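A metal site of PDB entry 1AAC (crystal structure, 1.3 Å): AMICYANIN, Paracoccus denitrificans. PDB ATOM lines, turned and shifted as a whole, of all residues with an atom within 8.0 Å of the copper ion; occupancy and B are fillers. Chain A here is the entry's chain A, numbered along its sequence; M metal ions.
A ring nitrogen (ND1) of His 53 sits close to the side-chain sulfur (SD) of Met 98, 3.3 Å away.
The backbone carbonyl oxygen (O) of Met 51 lies close to a ring nitrogen (NE2) of His 53 (3.5 Å).
OE2 of Glu 49 lies within hydrogen-bond range of NE2 of His 53 (2.7 Å).
The backbone NH of Met 72 is in hydrogen-bond range of the backbone carbonyl oxygen of His 53, 2.8 Å away.
N of Cys 92 is in hydrogen-bond range of O of Met 98, at 3.2 Å.
SG of Cys 92 lies close to OD1 of Asn 54 (3.6 Å).
The backbone NH (N) of Cys 92 is in hydrogen-bond range of the side-chain hydroxyl (OH) of Tyr 30.
Residues that only touch the copper ion: Pro 52 (3.9 Å).
Within 4 Å of the copper ion: Pro 52, His 53, Cys 92, His 95 and Met 98.
Along chain A the residues within 4 Å of the copper ion span positions 52 to 98.
The copper ion is bound by a ring nitrogen (ND1) of His 53, a ring nitrogen (ND1) of His 95 and the side-chain sulfur (SG) of Cys 92.
Slightly farther from the copper ion lies the side-chain sulfur (SD) of Met 98 (2.9 Å).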
ATOM      1  N   ILE A  25      -2.436  14.265   9.051  1.00  0.00           N
ATOM      2  CA  ILE A  25      -1.486  14.619   8.008  1.00  0.00           C
ATOM      3  C   ILE A  25      -0.218  13.864   8.367  1.00  0.00           C
ATOM      4  O   ILE A  25       0.301  14.021   9.474  1.00  0.00           O
ATOM      5  CB  ILE A  25      -1.209  16.144   7.989  1.00  0.00           C
ATOM      6  CG1 ILE A  25      -2.502  16.944   7.928  1.00  0.00           C
ATOM      7  CG2 ILE A  25      -0.294  16.422   6.799  1.00  0.00           C
ATOM      8  CD1 ILE A  25      -2.274  18.440   8.148  1.00  0.00           C
ATOM      9  N   MET A  28       3.802  13.394   4.241  1.00  0.00           N
ATOM     10  CA  MET A  28       3.550  14.447   3.258  1.00  0.00           C
ATOM     11  C   MET A  28       2.239  14.287   2.492  1.00  0.00           C
ATOM     12  O   MET A  28       2.156  14.601   1.285  1.00  0.00           O
ATOM     13  CB  MET A  28       4.731  14.514   2.251  1.00  0.00           C
ATOM     14  CG  MET A  28       6.090  14.773   2.886  1.00  0.00           C
ATOM     15  SD  MET A  28       6.269  16.339   3.789  1.00  0.00           S
ATOM     16  CE  MET A  28       6.150  17.472   2.457  1.00  0.00           C
ATOM     17  N   LYS A  29       1.180  13.759   3.137  1.00  0.00           N
ATOM     18  CA  LYS A  29      -0.110  13.646   2.483  1.00  0.00           C
ATOM     19  C   LYS A  29      -1.238  13.884   3.487  1.00  0.00           C
ATOM     20  O   LYS A  29      -1.046  13.730   4.703  1.00  0.00           O
ATOM     21  CB  LYS A  29      -0.331  12.225   1.946  1.00  0.00           C
ATOM     22  CG  LYS A  29       0.691  11.670   0.967  1.00  0.00           C
ATOM     23  CD  LYS A  29       0.565  10.168   0.789  1.00  0.00           C
ATOM     24  CE  LYS A  29       1.731   9.771  -0.092  1.00  0.00           C
ATOM     25  NZ  LYS A  29       1.896   8.343  -0.098  1.00  0.00           N
ATOM     26  N   TYR A  30      -2.396  14.342   3.003  1.00  0.00           N
ATOM     27  CA  TYR A  30      -3.579  14.367   3.844  1.00  0.00           C
ATOM     28  C   TYR A  30      -4.100  12.928   3.807  1.00  0.00           C
ATOM     29  O   TYR A  30      -4.382  12.375   2.713  1.00  0.00           O
ATOM     30  CB  TYR A  30      -4.638  15.321   3.267  1.00  0.00           C
ATOM     31  CG  TYR A  30      -4.143  16.762   3.221  1.00  0.00           C
ATOM     32  CD1 TYR A  30      -3.966  17.488   4.398  1.00  0.00           C
ATOM     33  CD2 TYR A  30      -3.879  17.354   1.983  1.00  0.00           C
ATOM     34  CE1 TYR A  30      -3.534  18.795   4.335  1.00  0.00           C
ATOM     35  CE2 TYR A  30      -3.456  18.660   1.915  1.00  0.00           C
ATOM     36  CZ  TYR A  30      -3.288  19.376   3.090  1.00  0.00           C
ATOM     37  OH  TYR A  30      -2.904  20.702   3.009  1.00  0.00           O
ATOM     38  N   ASN A  47      -1.537  17.579  12.396  1.00  0.00           N
ATOM     39  CA  ASN A  47      -0.254  17.274  11.790  1.00  0.00           C
ATOM     40  C   ASN A  47       0.454  16.249  12.683  1.00  0.00           C
ATOM     41  O   ASN A  47       0.743  16.523  13.861  1.00  0.00           O
ATOM     42  CB  ASN A  47       0.601  18.532  11.689  1.00  0.00           C
ATOM     43  CG  ASN A  47       1.870  18.270  10.878  1.00  0.00           C
ATOM     44  OD1 ASN A  47       2.070  17.169  10.334  1.00  0.00           O
ATOM     45  ND2 ASN A  47       2.763  19.234  10.775  1.00  0.00           N
ATOM     46  N   GLU A  49       3.413  14.825  11.798  1.00  0.00           N
ATOM     47  CA  GLU A  49       4.838  14.731  11.539  1.00  0.00           C
ATOM     48  C   GLU A  49       5.529  16.047  11.789  1.00  0.00           C
ATOM     49  O   GLU A  49       4.895  17.079  12.018  1.00  0.00           O
ATOM     50  CB  GLU A  49       5.046  14.238  10.120  1.00  0.00           C
ATOM     51  CG  GLU A  49       4.637  15.138   8.974  1.00  0.00           C
ATOM     52  CD  GLU A  49       4.870  14.501   7.609  1.00  0.00           C
ATOM     53  OE1 GLU A  49       5.553  13.476   7.507  1.00  0.00           O
ATOM     54  OE2 GLU A  49       4.351  15.007   6.636  1.00  0.00           O
ATOM     55  N   MET A  51       7.531  17.967   9.915  1.00  0.00           N
ATOM     56  CA  MET A  51       7.495  18.966   8.860  1.00  0.00           C
ATOM     57  C   MET A  51       6.205  19.768   8.973  1.00  0.00           C
ATOM     58  O   MET A  51       5.145  19.157   8.994  1.00  0.00           O
ATOM     59  CB  MET A  51       7.556  18.243   7.513  1.00  0.00           C
ATOM     60  CG  MET A  51       7.545  19.063   6.244  1.00  0.00           C
ATOM     61  SD  MET A  51       8.750  20.403   6.285  1.00  0.00           S
ATOM     62  CE  MET A  51      10.335  19.608   6.364  1.00  0.00           C
ATOM     63  N   PRO A  52       6.217  21.117   9.080  1.00  0.00           N
ATOM     64  CA  PRO A  52       5.007  21.908   9.214  1.00  0.00           C
ATOM     65  C   PRO A  52       4.109  21.839   7.982  1.00  0.00           C
ATOM     66  O   PRO A  52       4.600  21.821   6.848  1.00  0.00           O
ATOM     67  CB  PRO A  52       5.493  23.315   9.484  1.00  0.00           C
ATOM     68  CG  PRO A  52       6.825  23.059  10.161  1.00  0.00           C
ATOM     69  CD  PRO A  52       7.394  21.945   9.298  1.00  0.00           C
ATOM     70  N   HIS A  53       2.789  21.822   8.199  1.00  0.00           N
ATOM     71  CA  HIS A  53       1.829  21.779   7.091  1.00  0.00           C
ATOM     72  C   HIS A  53       0.652  22.679   7.465  1.00  0.00           C
ATOM     73  O   HIS A  53       0.483  22.996   8.641  1.00  0.00           O
ATOM     74  CB  HIS A  53       1.261  20.355   6.853  1.00  0.00           C
ATOM     75  CG  HIS A  53       2.270  19.289   6.430  1.00  0.00           C
ATOM     76  ND1 HIS A  53       2.830  19.303   5.241  1.00  0.00           N
ATOM     77  CD2 HIS A  53       2.653  18.223   7.194  1.00  0.00           C
ATOM     78  CE1 HIS A  53       3.585  18.232   5.223  1.00  0.00           C
ATOM     79  NE2 HIS A  53       3.488  17.596   6.373  1.00  0.00           N
ATOM     80  N   ASN A  54      -0.146  23.099   6.479  1.00  0.00           N
ATOM     81  CA  ASN A  54      -1.346  23.868   6.775  1.00  0.00           C
ATOM     82  C   ASN A  54      -2.389  23.402   5.769  1.00  0.00           C
ATOM     83  O   ASN A  54      -2.171  22.414   5.063  1.00  0.00           O
ATOM     84  CB  ASN A  54      -1.077  25.390   6.614  1.00  0.00           C
ATOM     85  CG  ASN A  54      -0.941  25.857   5.174  1.00  0.00           C
ATOM     86  OD1 ASN A  54      -0.571  25.099   4.271  1.00  0.00           O
ATOM     87  ND2 ASN A  54      -1.173  27.143   4.920  1.00  0.00           N
ATOM     88  N   VAL A  55      -3.554  24.050   5.758  1.00  0.00           N
ATOM     89  CA  VAL A  55      -4.560  23.876   4.734  1.00  0.00           C
ATOM     90  C   VAL A  55      -4.799  25.280   4.166  1.00  0.00           C
ATOM     91  O   VAL A  55      -4.810  26.281   4.902  1.00  0.00           O
ATOM     92  CB  VAL A  55      -5.887  23.269   5.278  1.00  0.00           C
ATOM     93  CG1 VAL A  55      -5.576  21.866   5.744  1.00  0.00           C
ATOM     94  CG2 VAL A  55      -6.486  24.047   6.441  1.00  0.00           C
ATOM     95  N   MET A  71       0.478  27.564   9.969  1.00  0.00           N
ATOM     96  CA  MET A  71       1.325  26.389   9.888  1.00  0.00           C
ATOM     97  C   MET A  71       1.222  25.609  11.204  1.00  0.00           C
ATOM     98  O   MET A  71       1.315  26.155  12.297  1.00  0.00           O
ATOM     99  CB  MET A  71       2.763  26.803   9.640  1.00  0.00           C
ATOM    100  CG  MET A  71       2.980  27.553   8.322  1.00  0.00           C
ATOM    101  SD  MET A  71       2.353  26.717   6.822  1.00  0.00           S
ATOM    102  CE  MET A  71       3.388  25.290   6.909  1.00  0.00           C
ATOM    103  N   MET A  72       0.948  24.311  11.102  1.00  0.00           N
ATOM    104  CA  MET A  72       0.794  23.418  12.238  1.00  0.00           C
ATOM    105  C   MET A  72       2.114  22.698  12.418  1.00  0.00           C
ATOM    106  O   MET A  72       2.628  22.075  11.479  1.00  0.00           O
ATOM    107  CB  MET A  72      -0.283  22.355  11.976  1.00  0.00           C
ATOM    108  CG  MET A  72      -1.714  22.866  12.044  1.00  0.00           C
ATOM    109  SD  MET A  72      -2.871  21.586  11.513  1.00  0.00           S
ATOM    110  CE  MET A  72      -2.897  22.087   9.831  1.00  0.00           C
ATOM    111  N   HIS A  91      -5.087  22.898  -0.525  1.00  0.00           N
ATOM    112  CA  HIS A  91      -3.761  22.354  -0.671  1.00  0.00           C
ATOM    113  C   HIS A  91      -2.910  22.834   0.500  1.00  0.00           C
ATOM    114  O   HIS A  91      -3.366  23.641   1.323  1.00  0.00           O
ATOM    115  CB  HIS A  91      -3.157  22.791  -2.017  1.00  0.00           C
ATOM    116  CG  HIS A  91      -2.922  24.285  -2.175  1.00  0.00           C
ATOM    117  ND1 HIS A  91      -3.839  25.190  -2.492  1.00  0.00           N
ATOM    118  CD2 HIS A  91      -1.725  24.945  -2.002  1.00  0.00           C
ATOM    119  CE1 HIS A  91      -3.255  26.363  -2.510  1.00  0.00           C
ATOM    120  NE2 HIS A  91      -1.976  26.222  -2.216  1.00  0.00           N
ATOM    121  N   CYS A  92      -1.674  22.372   0.574  1.00  0.00           N
ATOM    122  CA  CYS A  92      -0.739  22.821   1.600  1.00  0.00           C
ATOM    123  C   CYS A  92       0.096  23.940   0.985  1.00  0.00           C
ATOM    124  O   CYS A  92       0.767  23.708  -0.043  1.00  0.00           O
ATOM    125  CB  CYS A  92       0.118  21.656   2.019  1.00  0.00           C
ATOM    126  SG  CYS A  92       1.315  22.154   3.279  1.00  0.00           S
ATOM    127  N   THR A  93       0.140  25.150   1.540  1.00  0.00           N
ATOM    128  CA  THR A  93       0.871  26.259   0.933  1.00  0.00           C
ATOM    129  C   THR A  93       2.335  25.936   0.597  1.00  0.00           C
ATOM    130  O   THR A  93       2.680  26.153  -0.586  1.00  0.00           O
ATOM    131  CB  THR A  93       0.794  27.495   1.847  1.00  0.00           C
ATOM    132  OG1 THR A  93      -0.571  27.750   2.149  1.00  0.00           O
ATOM    133  CG2 THR A  93       1.400  28.728   1.165  1.00  0.00           C
ATOM    134  N   PRO A  94       3.246  25.460   1.471  1.00  0.00           N
ATOM    135  CA  PRO A  94       4.637  25.175   1.098  1.00  0.00           C
ATOM    136  C   PRO A  94       4.789  23.935   0.234  1.00  0.00           C
ATOM    137  O   PRO A  94       5.826  23.767  -0.431  1.00  0.00           O
ATOM    138  CB  PRO A  94       5.370  25.084   2.431  1.00  0.00           C
ATOM    139  CG  PRO A  94       4.292  24.548   3.369  1.00  0.00           C
ATOM    140  CD  PRO A  94       3.076  25.339   2.922  1.00  0.00           C
ATOM    141  N   HIS A  95       3.770  23.069   0.199  1.00  0.00           N
ATOM    142  CA  HIS A  95       3.859  21.776  -0.485  1.00  0.00           C
ATOM    143  C   HIS A  95       2.616  21.613  -1.366  1.00  0.00           C
ATOM    144  O   HIS A  95       1.746  20.798  -1.029  1.00  0.00           O
ATOM    145  CB  HIS A  95       3.921  20.627   0.557  1.00  0.00           C
ATOM    146  CG  HIS A  95       4.886  20.830   1.726  1.00  0.00           C
ATOM    147  ND1 HIS A  95       4.452  20.762   2.983  1.00  0.00           N
ATOM    148  CD2 HIS A  95       6.227  21.087   1.648  1.00  0.00           C
ATOM    149  CE1 HIS A  95       5.517  20.994   3.720  1.00  0.00           C
ATOM    150  NE2 HIS A  95       6.553  21.178   2.930  1.00  0.00           N
ATOM    151  N   PRO A  96       2.455  22.348  -2.479  1.00  0.00           N
ATOM    152  CA  PRO A  96       1.207  22.383  -3.235  1.00  0.00           C
ATOM    153  C   PRO A  96       0.856  21.077  -3.929  1.00  0.00           C
ATOM    154  O   PRO A  96      -0.237  20.905  -4.431  1.00  0.00           O
ATOM    155  CB  PRO A  96       1.393  23.546  -4.190  1.00  0.00           C
ATOM    156  CG  PRO A  96       2.871  23.643  -4.373  1.00  0.00           C
ATOM    157  CD  PRO A  96       3.393  23.356  -2.975  1.00  0.00           C
ATOM    158  N   PHE A  97       1.779  20.105  -3.959  1.00  0.00           N
ATOM    159  CA  PHE A  97       1.439  18.768  -4.443  1.00  0.00           C
ATOM    160  C   PHE A  97       0.528  18.020  -3.439  1.00  0.00           C
ATOM    161  O   PHE A  97      -0.052  16.993  -3.786  1.00  0.00           O
ATOM    162  CB  PHE A  97       2.748  17.983  -4.690  1.00  0.00           C
ATOM    163  CG  PHE A  97       3.726  17.968  -3.521  1.00  0.00           C
ATOM    164  CD1 PHE A  97       3.567  17.065  -2.465  1.00  0.00           C
ATOM    165  CD2 PHE A  97       4.763  18.890  -3.504  1.00  0.00           C
ATOM    166  CE1 PHE A  97       4.450  17.102  -1.405  1.00  0.00           C
ATOM    167  CE2 PHE A  97       5.632  18.919  -2.438  1.00  0.00           C
ATOM    168  CZ  PHE A  97       5.469  18.024  -1.397  1.00  0.00           C
ATOM    169  N   MET A  98       0.419  18.493  -2.197  1.00  0.00           N
ATOM    170  CA  MET A  98      -0.471  17.910  -1.184  1.00  0.00           C
ATOM    171  C   MET A  98      -1.837  18.548  -1.421  1.00  0.00           C
ATOM    172  O   MET A  98      -1.988  19.762  -1.196  1.00  0.00           O
ATOM    173  CB  MET A  98      -0.052  18.268   0.243  1.00  0.00           C
ATOM    174  CG  MET A  98       1.278  17.708   0.612  1.00  0.00           C
ATOM    175  SD  MET A  98       1.741  18.140   2.306  1.00  0.00           S
ATOM    176  CE  MET A  98       0.421  17.489   3.294  1.00  0.00           C
HETATM  177 CU    CU M   1       2.579  20.525   3.736  1.00  0.00          CU
